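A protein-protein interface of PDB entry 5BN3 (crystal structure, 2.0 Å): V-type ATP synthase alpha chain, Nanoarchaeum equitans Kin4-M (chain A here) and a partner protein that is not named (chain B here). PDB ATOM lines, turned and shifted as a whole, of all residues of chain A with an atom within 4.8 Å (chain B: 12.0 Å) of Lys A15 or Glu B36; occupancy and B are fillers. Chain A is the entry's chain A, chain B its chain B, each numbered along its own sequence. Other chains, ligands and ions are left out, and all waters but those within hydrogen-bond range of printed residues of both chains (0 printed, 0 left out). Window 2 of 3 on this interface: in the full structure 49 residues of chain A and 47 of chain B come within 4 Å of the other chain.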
ATOM      1  N   MET A   1     -29.023 -27.592 -22.241  1.00  0.00           N
ATOM      2  CA  MET A   1     -30.082 -26.603 -22.409  1.00  0.00           C
ATOM      3  C   MET A   1     -30.315 -25.820 -21.121  1.00  0.00           C
ATOM      4  O   MET A   1     -30.137 -24.602 -21.083  1.00  0.00           O
ATOM      5  CB  MET A   1     -31.366 -27.275 -22.863  1.00  0.00           C
ATOM      6  N   ASN A   2     -30.730 -26.523 -20.071  1.00  0.00           N
ATOM      7  CA  ASN A   2     -30.889 -25.907 -18.761  1.00  0.00           C
ATOM      8  C   ASN A   2     -29.545 -25.379 -18.260  1.00  0.00           C
ATOM      9  O   ASN A   2     -28.526 -26.060 -18.373  1.00  0.00           O
ATOM     10  CB  ASN A   2     -31.451 -26.915 -17.757  1.00  0.00           C
ATOM     11  CG  ASN A   2     -32.731 -27.574 -18.239  1.00  0.00           C
ATOM     12  OD1 ASN A   2     -33.590 -26.929 -18.840  1.00  0.00           O
ATOM     13  ND2 ASN A   2     -32.864 -28.869 -17.971  1.00  0.00           N
ATOM     14  N   ARG A   3     -29.542 -24.166 -17.716  1.00  0.00           N
ATOM     15  CA  ARG A   3     -28.298 -23.553 -17.260  1.00  0.00           C
ATOM     16  C   ARG A   3     -28.452 -22.837 -15.921  1.00  0.00           C
ATOM     17  O   ARG A   3     -29.485 -22.224 -15.651  1.00  0.00           O
ATOM     18  CB  ARG A   3     -27.762 -22.594 -18.316  1.00  0.00           C
ATOM     19  N   ILE A   5     -28.004 -19.841 -13.465  1.00  0.00           N
ATOM     20  CA  ILE A   5     -27.875 -18.395 -13.629  1.00  0.00           C
ATOM     21  C   ILE A   5     -27.470 -17.722 -12.319  1.00  0.00           C
ATOM     22  O   ILE A   5     -27.139 -16.535 -12.297  1.00  0.00           O
ATOM     23  CB  ILE A   5     -29.164 -17.746 -14.176  1.00  0.00           C
ATOM     24  CG1 ILE A   5     -30.262 -17.742 -13.115  1.00  0.00           C
ATOM     25  CG2 ILE A   5     -29.630 -18.453 -15.444  1.00  0.00           C
ATOM     26  CD1 ILE A   5     -31.456 -16.894 -13.490  1.00  0.00           C
ATOM     27  N   ILE A  13     -30.129 -21.211  -8.753  1.00  0.00           N
ATOM     28  CA  ILE A  13     -31.197 -20.792  -9.652  1.00  0.00           C
ATOM     29  C   ILE A  13     -30.813 -21.157 -11.082  1.00  0.00           C
ATOM     30  O   ILE A  13     -29.706 -20.848 -11.535  1.00  0.00           O
ATOM     31  CB  ILE A  13     -31.482 -19.280  -9.544  1.00  0.00           C
ATOM     32  CG1 ILE A  13     -31.887 -18.924  -8.111  1.00  0.00           C
ATOM     33  CG2 ILE A  13     -32.585 -18.867 -10.508  1.00  0.00           C
ATOM     34  CD1 ILE A  13     -32.038 -17.436  -7.859  1.00  0.00           C
ATOM     35  N   ALA A  14     -31.721 -21.827 -11.784  1.00  0.00           N
ATOM     36  CA  ALA A  14     -31.457 -22.266 -13.149  1.00  0.00           C
ATOM     37  C   ALA A  14     -32.566 -21.853 -14.106  1.00  0.00           C
ATOM     38  O   ALA A  14     -33.741 -21.834 -13.736  1.00  0.00           O
ATOM     39  CB  ALA A  14     -31.265 -23.775 -13.191  1.00  0.00           C
ATOM     40  N   LYS A  15     -32.187 -21.520 -15.337  1.00  0.00           N
ATOM     41  CA  LYS A  15     -33.160 -21.309 -16.402  1.00  0.00           C
ATOM     42  C   LYS A  15     -33.377 -22.620 -17.146  1.00  0.00           C
ATOM     43  O   LYS A  15     -32.429 -23.375 -17.373  1.00  0.00           O
ATOM     44  CB  LYS A  15     -32.676 -20.238 -17.384  1.00  0.00           C
ATOM     45  CG  LYS A  15     -33.142 -18.822 -17.073  1.00  0.00           C
ATOM     46  CD  LYS A  15     -33.067 -17.955 -18.327  1.00  0.00           C
ATOM     47  CE  LYS A  15     -33.561 -16.535 -18.079  1.00  0.00           C
ATOM     48  NZ  LYS A  15     -32.516 -15.656 -17.489  1.00  0.00           N
ATOM     49  N   GLY A  16     -34.623 -22.891 -17.523  1.00  0.00           N
ATOM     50  CA  GLY A  16     -34.937 -24.096 -18.268  1.00  0.00           C
ATOM     51  C   GLY A  16     -36.331 -24.630 -18.005  1.00  0.00           C
ATOM     52  O   GLY A  16     -37.220 -23.890 -17.576  1.00  0.00           O
ATOM     53  N   LYS A  17     -36.526 -25.918 -18.271  1.00  0.00           N
ATOM     54  CA  LYS A  17     -37.809 -26.568 -18.029  1.00  0.00           C
ATOM     55  C   LYS A  17     -37.688 -27.581 -16.896  1.00  0.00           C
ATOM     56  O   LYS A  17     -36.904 -28.530 -16.980  1.00  0.00           O
ATOM     57  CB  LYS A  17     -38.307 -27.247 -19.294  1.00  0.00           C
ATOM     58  N   PHE A  18     -38.469 -27.383 -15.840  1.00  0.00           N
ATOM     59  CA  PHE A  18     -38.394 -28.249 -14.668  1.00  0.00           C
ATOM     60  C   PHE A  18     -39.774 -28.549 -14.093  1.00  0.00           C
ATOM     61  O   PHE A  18     -40.760 -27.907 -14.453  1.00  0.00           O
ATOM     62  CB  PHE A  18     -37.525 -27.600 -13.587  1.00  0.00           C
ATOM     63  CG  PHE A  18     -36.108 -27.341 -14.015  1.00  0.00           C
ATOM     64  CD1 PHE A  18     -35.138 -28.319 -13.870  1.00  0.00           C
ATOM     65  CD2 PHE A  18     -35.744 -26.116 -14.552  1.00  0.00           C
ATOM     66  CE1 PHE A  18     -33.830 -28.081 -14.255  1.00  0.00           C
ATOM     67  CE2 PHE A  18     -34.437 -25.870 -14.937  1.00  0.00           C
ATOM     68  CZ  PHE A  18     -33.480 -26.856 -14.790  1.00  0.00           C
ATOM     69  N   ASP A  41     -39.593 -19.225 -16.182  1.00  0.00           N
ATOM     70  CA  ASP A  41     -38.573 -20.060 -16.805  1.00  0.00           C
ATOM     71  C   ASP A  41     -37.457 -20.420 -15.828  1.00  0.00           C
ATOM     72  O   ASP A  41     -36.524 -21.151 -16.175  1.00  0.00           O
ATOM     73  CB  ASP A  41     -37.987 -19.346 -18.022  1.00  0.00           C
ATOM     74  CG  ASP A  41     -37.629 -17.900 -17.731  1.00  0.00           C
ATOM     75  OD1 ASP A  41     -38.290 -17.283 -16.869  1.00  0.00           O
ATOM     76  OD2 ASP A  41     -36.691 -17.380 -18.367  1.00  0.00           O
ATOM     77  N   LYS A  42     -37.560 -19.905 -14.608  1.00  0.00           N
ATOM     78  CA  LYS A  42     -36.544 -20.135 -13.588  1.00  0.00           C
ATOM     79  C   LYS A  42     -36.940 -21.257 -12.635  1.00  0.00           C
ATOM     80  O   LYS A  42     -38.123 -21.460 -12.355  1.00  0.00           O
ATOM     81  CB  LYS A  42     -36.308 -18.857 -12.781  1.00  0.00           C
ATOM     82  CG  LYS A  42     -36.061 -17.618 -13.620  1.00  0.00           C
ATOM     83  CD  LYS A  42     -36.096 -16.375 -12.747  1.00  0.00           C
ATOM     84  CE  LYS A  42     -34.795 -15.595 -12.829  1.00  0.00           C
ATOM     85  NZ  LYS A  42     -34.651 -14.859 -14.112  1.00  0.00           N
ATOM     86  N   VAL A  56     -21.664 -20.134 -13.200  1.00  0.00           N
ATOM     87  CA  VAL A  56     -22.865 -19.693 -13.910  1.00  0.00           C
ATOM     88  C   VAL A  56     -22.909 -20.318 -15.311  1.00  0.00           C
ATOM     89  O   VAL A  56     -23.979 -20.557 -15.873  1.00  0.00           O
ATOM     90  CB  VAL A  56     -22.945 -18.144 -13.965  1.00  0.00           C
ATOM     91  CG1 VAL A  56     -24.014 -17.668 -14.937  1.00  0.00           C
ATOM     92  CG2 VAL A  56     -23.220 -17.582 -12.575  1.00  0.00           C
ATOM     93  N   ALA B  10     -17.527  -4.592  -6.827  1.00  0.00           N
ATOM     94  CA  ALA B  10     -18.556  -5.168  -7.684  1.00  0.00           C
ATOM     95  C   ALA B  10     -18.014  -5.177  -9.102  1.00  0.00           C
ATOM     96  O   ALA B  10     -17.489  -4.166  -9.579  1.00  0.00           O
ATOM     97  CB  ALA B  10     -19.835  -4.367  -7.609  1.00  0.00           C
ATOM     98  N   VAL B  11     -18.143  -6.312  -9.779  1.00  0.00           N
ATOM     99  CA  VAL B  11     -17.447  -6.494 -11.043  1.00  0.00           C
ATOM    100  C   VAL B  11     -18.221  -7.336 -12.063  1.00  0.00           C
ATOM    101  O   VAL B  11     -19.006  -8.212 -11.698  1.00  0.00           O
ATOM    102  CB  VAL B  11     -16.031  -7.057 -10.785  1.00  0.00           C
ATOM    103  CG1 VAL B  11     -15.815  -8.379 -11.497  1.00  0.00           C
ATOM    104  CG2 VAL B  11     -14.987  -6.031 -11.179  1.00  0.00           C
ATOM    105  N   GLU B  12     -18.003  -7.047 -13.344  1.00  0.00           N
ATOM    106  CA  GLU B  12     -18.686  -7.754 -14.421  1.00  0.00           C
ATOM    107  C   GLU B  12     -17.811  -8.892 -14.938  1.00  0.00           C
ATOM    108  O   GLU B  12     -16.684  -8.665 -15.383  1.00  0.00           O
ATOM    109  CB  GLU B  12     -19.021  -6.792 -15.566  1.00  0.00           C
ATOM    110  CG  GLU B  12     -19.521  -5.416 -15.124  1.00  0.00           C
ATOM    111  CD  GLU B  12     -18.395  -4.455 -14.764  1.00  0.00           C
ATOM    112  OE1 GLU B  12     -17.218  -4.877 -14.759  1.00  0.00           O
ATOM    113  OE2 GLU B  12     -18.688  -3.271 -14.485  1.00  0.00           O
ATOM    114  N   LEU B  13     -18.329 -10.116 -14.870  1.00  0.00           N
ATOM    115  CA  LEU B  13     -17.588 -11.296 -15.309  1.00  0.00           C
ATOM    116  C   LEU B  13     -18.457 -12.205 -16.169  1.00  0.00           C
ATOM    117  O   LEU B  13     -19.628 -12.425 -15.864  1.00  0.00           O
ATOM    118  CB  LEU B  13     -17.081 -12.096 -14.104  1.00  0.00           C
ATOM    119  CG  LEU B  13     -16.033 -11.496 -13.170  1.00  0.00           C
ATOM    120  CD1 LEU B  13     -15.700 -12.461 -12.042  1.00  0.00           C
ATOM    121  CD2 LEU B  13     -14.780 -11.138 -13.935  1.00  0.00           C
ATOM    122  N   GLU B  14     -17.880 -12.740 -17.239  1.00  0.00           N
ATOM    123  CA  GLU B  14     -18.560 -13.761 -18.025  1.00  0.00           C
ATOM    124  C   GLU B  14     -18.523 -15.076 -17.258  1.00  0.00           C
ATOM    125  O   GLU B  14     -17.447 -15.601 -16.969  1.00  0.00           O
ATOM    126  CB  GLU B  14     -17.900 -13.919 -19.381  1.00  0.00           C
ATOM    127  N   ASN B  15     -19.704 -15.595 -16.928  1.00  0.00           N
ATOM    128  CA  ASN B  15     -19.845 -16.841 -16.170  1.00  0.00           C
ATOM    129  C   ASN B  15     -19.017 -16.911 -14.881  1.00  0.00           C
ATOM    130  O   ASN B  15     -18.050 -17.670 -14.800  1.00  0.00           O
ATOM    131  CB  ASN B  15     -19.558 -18.054 -17.061  1.00  0.00           C
ATOM    132  CG  ASN B  15     -20.534 -18.171 -18.218  1.00  0.00           C
ATOM    133  OD1 ASN B  15     -21.596 -17.545 -18.221  1.00  0.00           O
ATOM    134  ND2 ASN B  15     -20.181 -18.984 -19.206  1.00  0.00           N
ATOM    135  N   PRO B  16     -19.407 -16.124 -13.866  1.00  0.00           N
ATOM    136  CA  PRO B  16     -18.687 -16.082 -12.587  1.00  0.00           C
ATOM    137  C   PRO B  16     -18.719 -17.423 -11.861  1.00  0.00           C
ATOM    138  O   PRO B  16     -19.719 -18.141 -11.934  1.00  0.00           O
ATOM    139  CB  PRO B  16     -19.474 -15.049 -11.775  1.00  0.00           C
ATOM    140  CG  PRO B  16     -20.218 -14.240 -12.787  1.00  0.00           C
ATOM    141  CD  PRO B  16     -20.550 -15.200 -13.883  1.00  0.00           C
ATOM    142  N   MET B  17     -17.630 -17.747 -11.171  1.00  0.00           N
ATOM    143  CA  MET B  17     -17.553 -18.959 -10.365  1.00  0.00           C
ATOM    144  C   MET B  17     -17.582 -18.587  -8.888  1.00  0.00           C
ATOM    145  O   MET B  17     -16.838 -17.711  -8.450  1.00  0.00           O
ATOM    146  CB  MET B  17     -16.268 -19.729 -10.686  1.00  0.00           C
ATOM    147  CG  MET B  17     -15.929 -20.846  -9.705  1.00  0.00           C
ATOM    148  SD  MET B  17     -14.260 -21.495  -9.950  1.00  0.00           S
ATOM    149  CE  MET B  17     -14.371 -22.072 -11.645  1.00  0.00           C
ATOM    150  N   LEU B  18     -18.447 -19.246  -8.125  1.00  0.00           N
ATOM    151  CA  LEU B  18     -18.539 -19.001  -6.689  1.00  0.00           C
ATOM    152  C   LEU B  18     -17.233 -19.409  -6.007  1.00  0.00           C
ATOM    153  O   LEU B  18     -16.804 -20.558  -6.117  1.00  0.00           O
ATOM    154  CB  LEU B  18     -19.701 -19.796  -6.091  1.00  0.00           C
ATOM    155  CG  LEU B  18     -20.584 -19.152  -5.017  1.00  0.00           C
ATOM    156  CD1 LEU B  18     -20.912 -20.165  -3.927  1.00  0.00           C
ATOM    157  CD2 LEU B  18     -19.953 -17.899  -4.427  1.00  0.00           C
ATOM    158  N   GLU B  20     -14.287 -18.067  -6.671  1.00  0.00           N
ATOM    159  CA  GLU B  20     -13.193 -17.910  -7.630  1.00  0.00           C
ATOM    160  C   GLU B  20     -12.164 -16.860  -7.198  1.00  0.00           C
ATOM    161  O   GLU B  20     -12.525 -15.775  -6.738  1.00  0.00           O
ATOM    162  CB  GLU B  20     -13.778 -17.542  -8.999  1.00  0.00           C
ATOM    163  CG  GLU B  20     -12.780 -17.294 -10.113  1.00  0.00           C
ATOM    164  CD  GLU B  20     -13.462 -16.893 -11.411  1.00  0.00           C
ATOM    165  OE1 GLU B  20     -12.837 -17.034 -12.481  1.00  0.00           O
ATOM    166  OE2 GLU B  20     -14.627 -16.434 -11.362  1.00  0.00           O
ATOM    167  N   VAL B  31     -14.379 -14.128  -5.235  1.00  0.00           N
ATOM    168  CA  VAL B  31     -15.769 -13.918  -5.630  1.00  0.00           C
ATOM    169  C   VAL B  31     -16.692 -14.544  -4.586  1.00  0.00           C
ATOM    170  O   VAL B  31     -16.644 -15.751  -4.355  1.00  0.00           O
ATOM    171  CB  VAL B  31     -16.063 -14.524  -7.016  1.00  0.00           C
ATOM    172  CG1 VAL B  31     -17.533 -14.378  -7.359  1.00  0.00           C
ATOM    173  CG2 VAL B  31     -15.205 -13.852  -8.077  1.00  0.00           C
ATOM    174  N   ILE B  32     -17.524 -13.720  -3.956  1.00  0.00           N
ATOM    175  CA  ILE B  32     -18.398 -14.189  -2.883  1.00  0.00           C
ATOM    176  C   ILE B  32     -19.868 -14.241  -3.300  1.00  0.00           C
ATOM    177  O   ILE B  32     -20.706 -14.772  -2.572  1.00  0.00           O
ATOM    178  CB  ILE B  32     -18.257 -13.324  -1.612  1.00  0.00           C
ATOM    179  CG1 ILE B  32     -18.583 -11.861  -1.920  1.00  0.00           C
ATOM    180  CG2 ILE B  32     -16.859 -13.448  -1.032  1.00  0.00           C
ATOM    181  CD1 ILE B  32     -18.609 -10.963  -0.695  1.00  0.00           C
ATOM    182  N   ALA B  33     -20.180 -13.682  -4.465  1.00  0.00           N
ATOM    183  CA  ALA B  33     -21.547 -13.714  -4.983  1.00  0.00           C
ATOM    184  C   ALA B  33     -21.560 -13.712  -6.508  1.00  0.00           C
ATOM    185  O   ALA B  33     -20.692 -13.106  -7.139  1.00  0.00           O
ATOM    186  CB  ALA B  33     -22.349 -12.544  -4.448  1.00  0.00           C
ATOM    187  N   ALA B  34     -22.550 -14.381  -7.096  1.00  0.00           N
ATOM    188  CA  ALA B  34     -22.640 -14.487  -8.550  1.00  0.00           C
ATOM    189  C   ALA B  34     -24.073 -14.630  -9.057  1.00  0.00           C
ATOM    190  O   ALA B  34     -24.747 -15.618  -8.761  1.00  0.00           O
ATOM    191  CB  ALA B  34     -21.796 -15.654  -9.040  1.00  0.00           C
ATOM    192  N   TYR B  35     -24.529 -13.640  -9.820  1.00  0.00           N
ATOM    193  CA  TYR B  35     -25.813 -13.717 -10.512  1.00  0.00           C
ATOM    194  C   TYR B  35     -25.610 -13.285 -11.961  1.00  0.00           C
ATOM    195  O   TYR B  35     -25.121 -12.181 -12.218  1.00  0.00           O
ATOM    196  CB  TYR B  35     -26.861 -12.822  -9.841  1.00  0.00           C
ATOM    197  CG  TYR B  35     -28.279 -13.120 -10.284  1.00  0.00           C
ATOM    198  CD1 TYR B  35     -28.783 -12.605 -11.471  1.00  0.00           C
ATOM    199  CD2 TYR B  35     -29.111 -13.920  -9.517  1.00  0.00           C
ATOM    200  CE1 TYR B  35     -30.078 -12.885 -11.881  1.00  0.00           C
ATOM    201  CE2 TYR B  35     -30.404 -14.208  -9.918  1.00  0.00           C
ATOM    202  CZ  TYR B  35     -30.882 -13.686 -11.100  1.00  0.00           C
ATOM    203  OH  TYR B  35     -32.168 -13.965 -11.502  1.00  0.00           O
ATOM    204  N   GLU B  36     -25.995 -14.154 -12.895  1.00  0.00           N
ATOM    205  CA  GLU B  36     -25.740 -13.942 -14.321  1.00  0.00           C
ATOM    206  C   GLU B  36     -24.280 -13.585 -14.569  1.00  0.00           C
ATOM    207  O   GLU B  36     -23.399 -14.421 -14.393  1.00  0.00           O
ATOM    208  CB  GLU B  36     -26.658 -12.861 -14.906  1.00  0.00           C
ATOM    209  CG  GLU B  36     -28.153 -13.155 -14.810  1.00  0.00           C
ATOM    210  CD  GLU B  36     -28.640 -14.187 -15.815  1.00  0.00           C
ATOM    211  OE1 GLU B  36     -27.805 -14.875 -16.438  1.00  0.00           O
ATOM    212  OE2 GLU B  36     -29.873 -14.307 -15.981  1.00  0.00           O
ATOM    213  N   ASN B  37     -24.029 -12.338 -14.961  1.00  0.00           N
ATOM    214  CA  ASN B  37     -22.665 -11.874 -15.206  1.00  0.00           C
ATOM    215  C   ASN B  37     -22.189 -10.834 -14.192  1.00  0.00           C
ATOM    216  O   ASN B  37     -21.201 -10.132 -14.425  1.00  0.00           O
ATOM    217  CB  ASN B  37     -22.520 -11.328 -16.630  1.00  0.00           C
ATOM    218  CG  ASN B  37     -23.430 -10.148 -16.900  1.00  0.00           C
ATOM    219  OD1 ASN B  37     -24.612 -10.171 -16.556  1.00  0.00           O
ATOM    220  ND2 ASN B  37     -22.883  -9.105 -17.517  1.00  0.00           N
ATOM    221  N   LYS B  38     -22.891 -10.742 -13.067  1.00  0.00           N
ATOM    222  CA  LYS B  38     -22.504  -9.832 -11.996  1.00  0.00           C
ATOM    223  C   LYS B  38     -21.816 -10.595 -10.869  1.00  0.00           C
ATOM    224  O   LYS B  38     -22.284 -11.656 -10.448  1.00  0.00           O
ATOM    225  CB  LYS B  38     -23.726  -9.094 -11.444  1.00  0.00           C
ATOM    226  CG  LYS B  38     -24.557  -8.364 -12.490  1.00  0.00           C
ATOM    227  CD  LYS B  38     -23.745  -7.310 -13.224  1.00  0.00           C
ATOM    228  CE  LYS B  38     -24.626  -6.477 -14.147  1.00  0.00           C
ATOM    229  NZ  LYS B  38     -25.417  -7.322 -15.084  1.00  0.00           N
ATOM    230  N   ALA B  39     -20.703 -10.056 -10.382  1.00  0.00           N
ATOM    231  CA  ALA B  39     -19.981 -10.676  -9.276  1.00  0.00           C
ATOM    232  C   ALA B  39     -19.628  -9.665  -8.192  1.00  0.00           C
ATOM    233  O   ALA B  39     -19.365  -8.496  -8.480  1.00  0.00           O
ATOM    234  CB  ALA B  39     -18.724 -11.362  -9.778  1.00  0.00           C
ATOM    235  N   LEU B  40     -19.631 -10.124  -6.946  1.00  0.00           N
ATOM    236  CA  LEU B  40     -19.105  -9.336  -5.840  1.00  0.00           C
ATOM    237  C   LEU B  40     -17.836 -10.027  -5.361  1.00  0.00           C
ATOM    238  O   LEU B  40     -17.802 -11.253  -5.247  1.00  0.00           O
ATOM    239  CB  LEU B  40     -20.118  -9.241  -4.696  1.00  0.00           C
ATOM    240  CG  LEU B  40     -21.463  -8.562  -4.969  1.00  0.00           C
ATOM    241  CD1 LEU B  40     -22.282  -8.414  -3.690  1.00  0.00           C
ATOM    242  CD2 LEU B  40     -21.265  -7.211  -5.629  1.00  0.00           C
ATOM    243  N   ARG B  56      -8.574 -13.976 -14.215  1.00  0.00           N
ATOM    244  CA  ARG B  56      -9.253 -15.034 -13.472  1.00  0.00           C
ATOM    245  C   ARG B  56      -8.401 -16.297 -13.411  1.00  0.00           C
ATOM    246  O   ARG B  56      -7.962 -16.809 -14.445  1.00  0.00           O
ATOM    247  CB  ARG B  56     -10.613 -15.342 -14.111  1.00  0.00           C
ATOM    248  CG  ARG B  56     -11.522 -14.126 -14.260  1.00  0.00           C
ATOM    249  CD  ARG B  56     -12.787 -14.444 -15.052  1.00  0.00           C
ATOM    250  NE  ARG B  56     -13.672 -15.373 -14.352  1.00  0.00           N
ATOM    251  CZ  ARG B  56     -14.867 -15.753 -14.797  1.00  0.00           C
ATOM    252  NH1 ARG B  56     -15.331 -15.285 -15.947  1.00  0.00           N
ATOM    253  NH2 ARG B  56     -15.600 -16.601 -14.090  1.00  0.00           N
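The backbone NH of Glu B36 is in hydrogen-bond range of the backbone carbonyl oxygen of Ile A5, at 2.7 Å.
NZ of Lys A15 is in salt-bridge range of OE2 of Glu B36 (3.3 Å).
The backbone carbonyl oxygen (O) of Pro B16 sits at hydrogen-bond distance from the backbone NH (N) of Val A56, 3.1 Å away.
O of Arg A3 is in hydrogen-bond range of N of Lys A15 (2.8 Å).
The backbone NH of Ile A5 sits at hydrogen-bond distance from the backbone carbonyl oxygen of Ile A13, at 2.8 Å.
Among the printed residues, pairs that only touch across the chains: Val A56 with Glu B36 (3.3 Å), Lys A42 with Tyr B35 (3.4 Å) and Ile A5 with Tyr B35 (3.6 Å).
No residue of chain B comes within 4 Å of Met A1.
Asn A2 touches none of the printed residues of chain B.
Arg A3 touches none of the printed residues of chain B.
Of chain B, only Tyr B35 (3.6 Å) and Glu B36 (2.7 Å) come within 4 Å of Ile A5.
Lys A15 touches just one residue of chain B: Glu B36 (3.3 Å).
No residue of chain B comes within 4 Å of Gly A16.
No residue of chain B comes within 4 Å of Lys A17.
No residue of chain B comes within 4 Å of Asp A41.
Lys A42 touches one residue of chain B.
Of chain B, only Pro B16 and Glu B36 come within 4 Å of Val A56.
Of the printed residues of chain A, Pro B16 touches Val A56 (3.1 Å).
Of the printed residues of chain A, Tyr B35 touches Ile A5 (3.6 Å) and Lys A42 (3.4 Å).
Asn B37 touches none of the printed residues of chain A.
Arg B56 touches none of the printed residues of chain A.
The nearest residue of chain B that does not touch Lys A15 is Tyr B35 (6.2 Å).
The nearest printed residue of chain A that does not touch Tyr B35 is Ile A13 (4.2 Å).
Of the 21 printed residues of chain B, 3 touch a printed residue of chain A.
Printed residues of chain B that touch a printed residue of chain A: Pro B16, Tyr B35 and Glu B36.
Of the 13 printed residues of chain A, 4 touch a printed residue of chain B.
Among the printed residues, Asp or Glu carboxylates within 4 Å of a Lys or Arg side-chain nitrogen of the other chain: Lys A15 with Glu B36 (3.3 Å).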
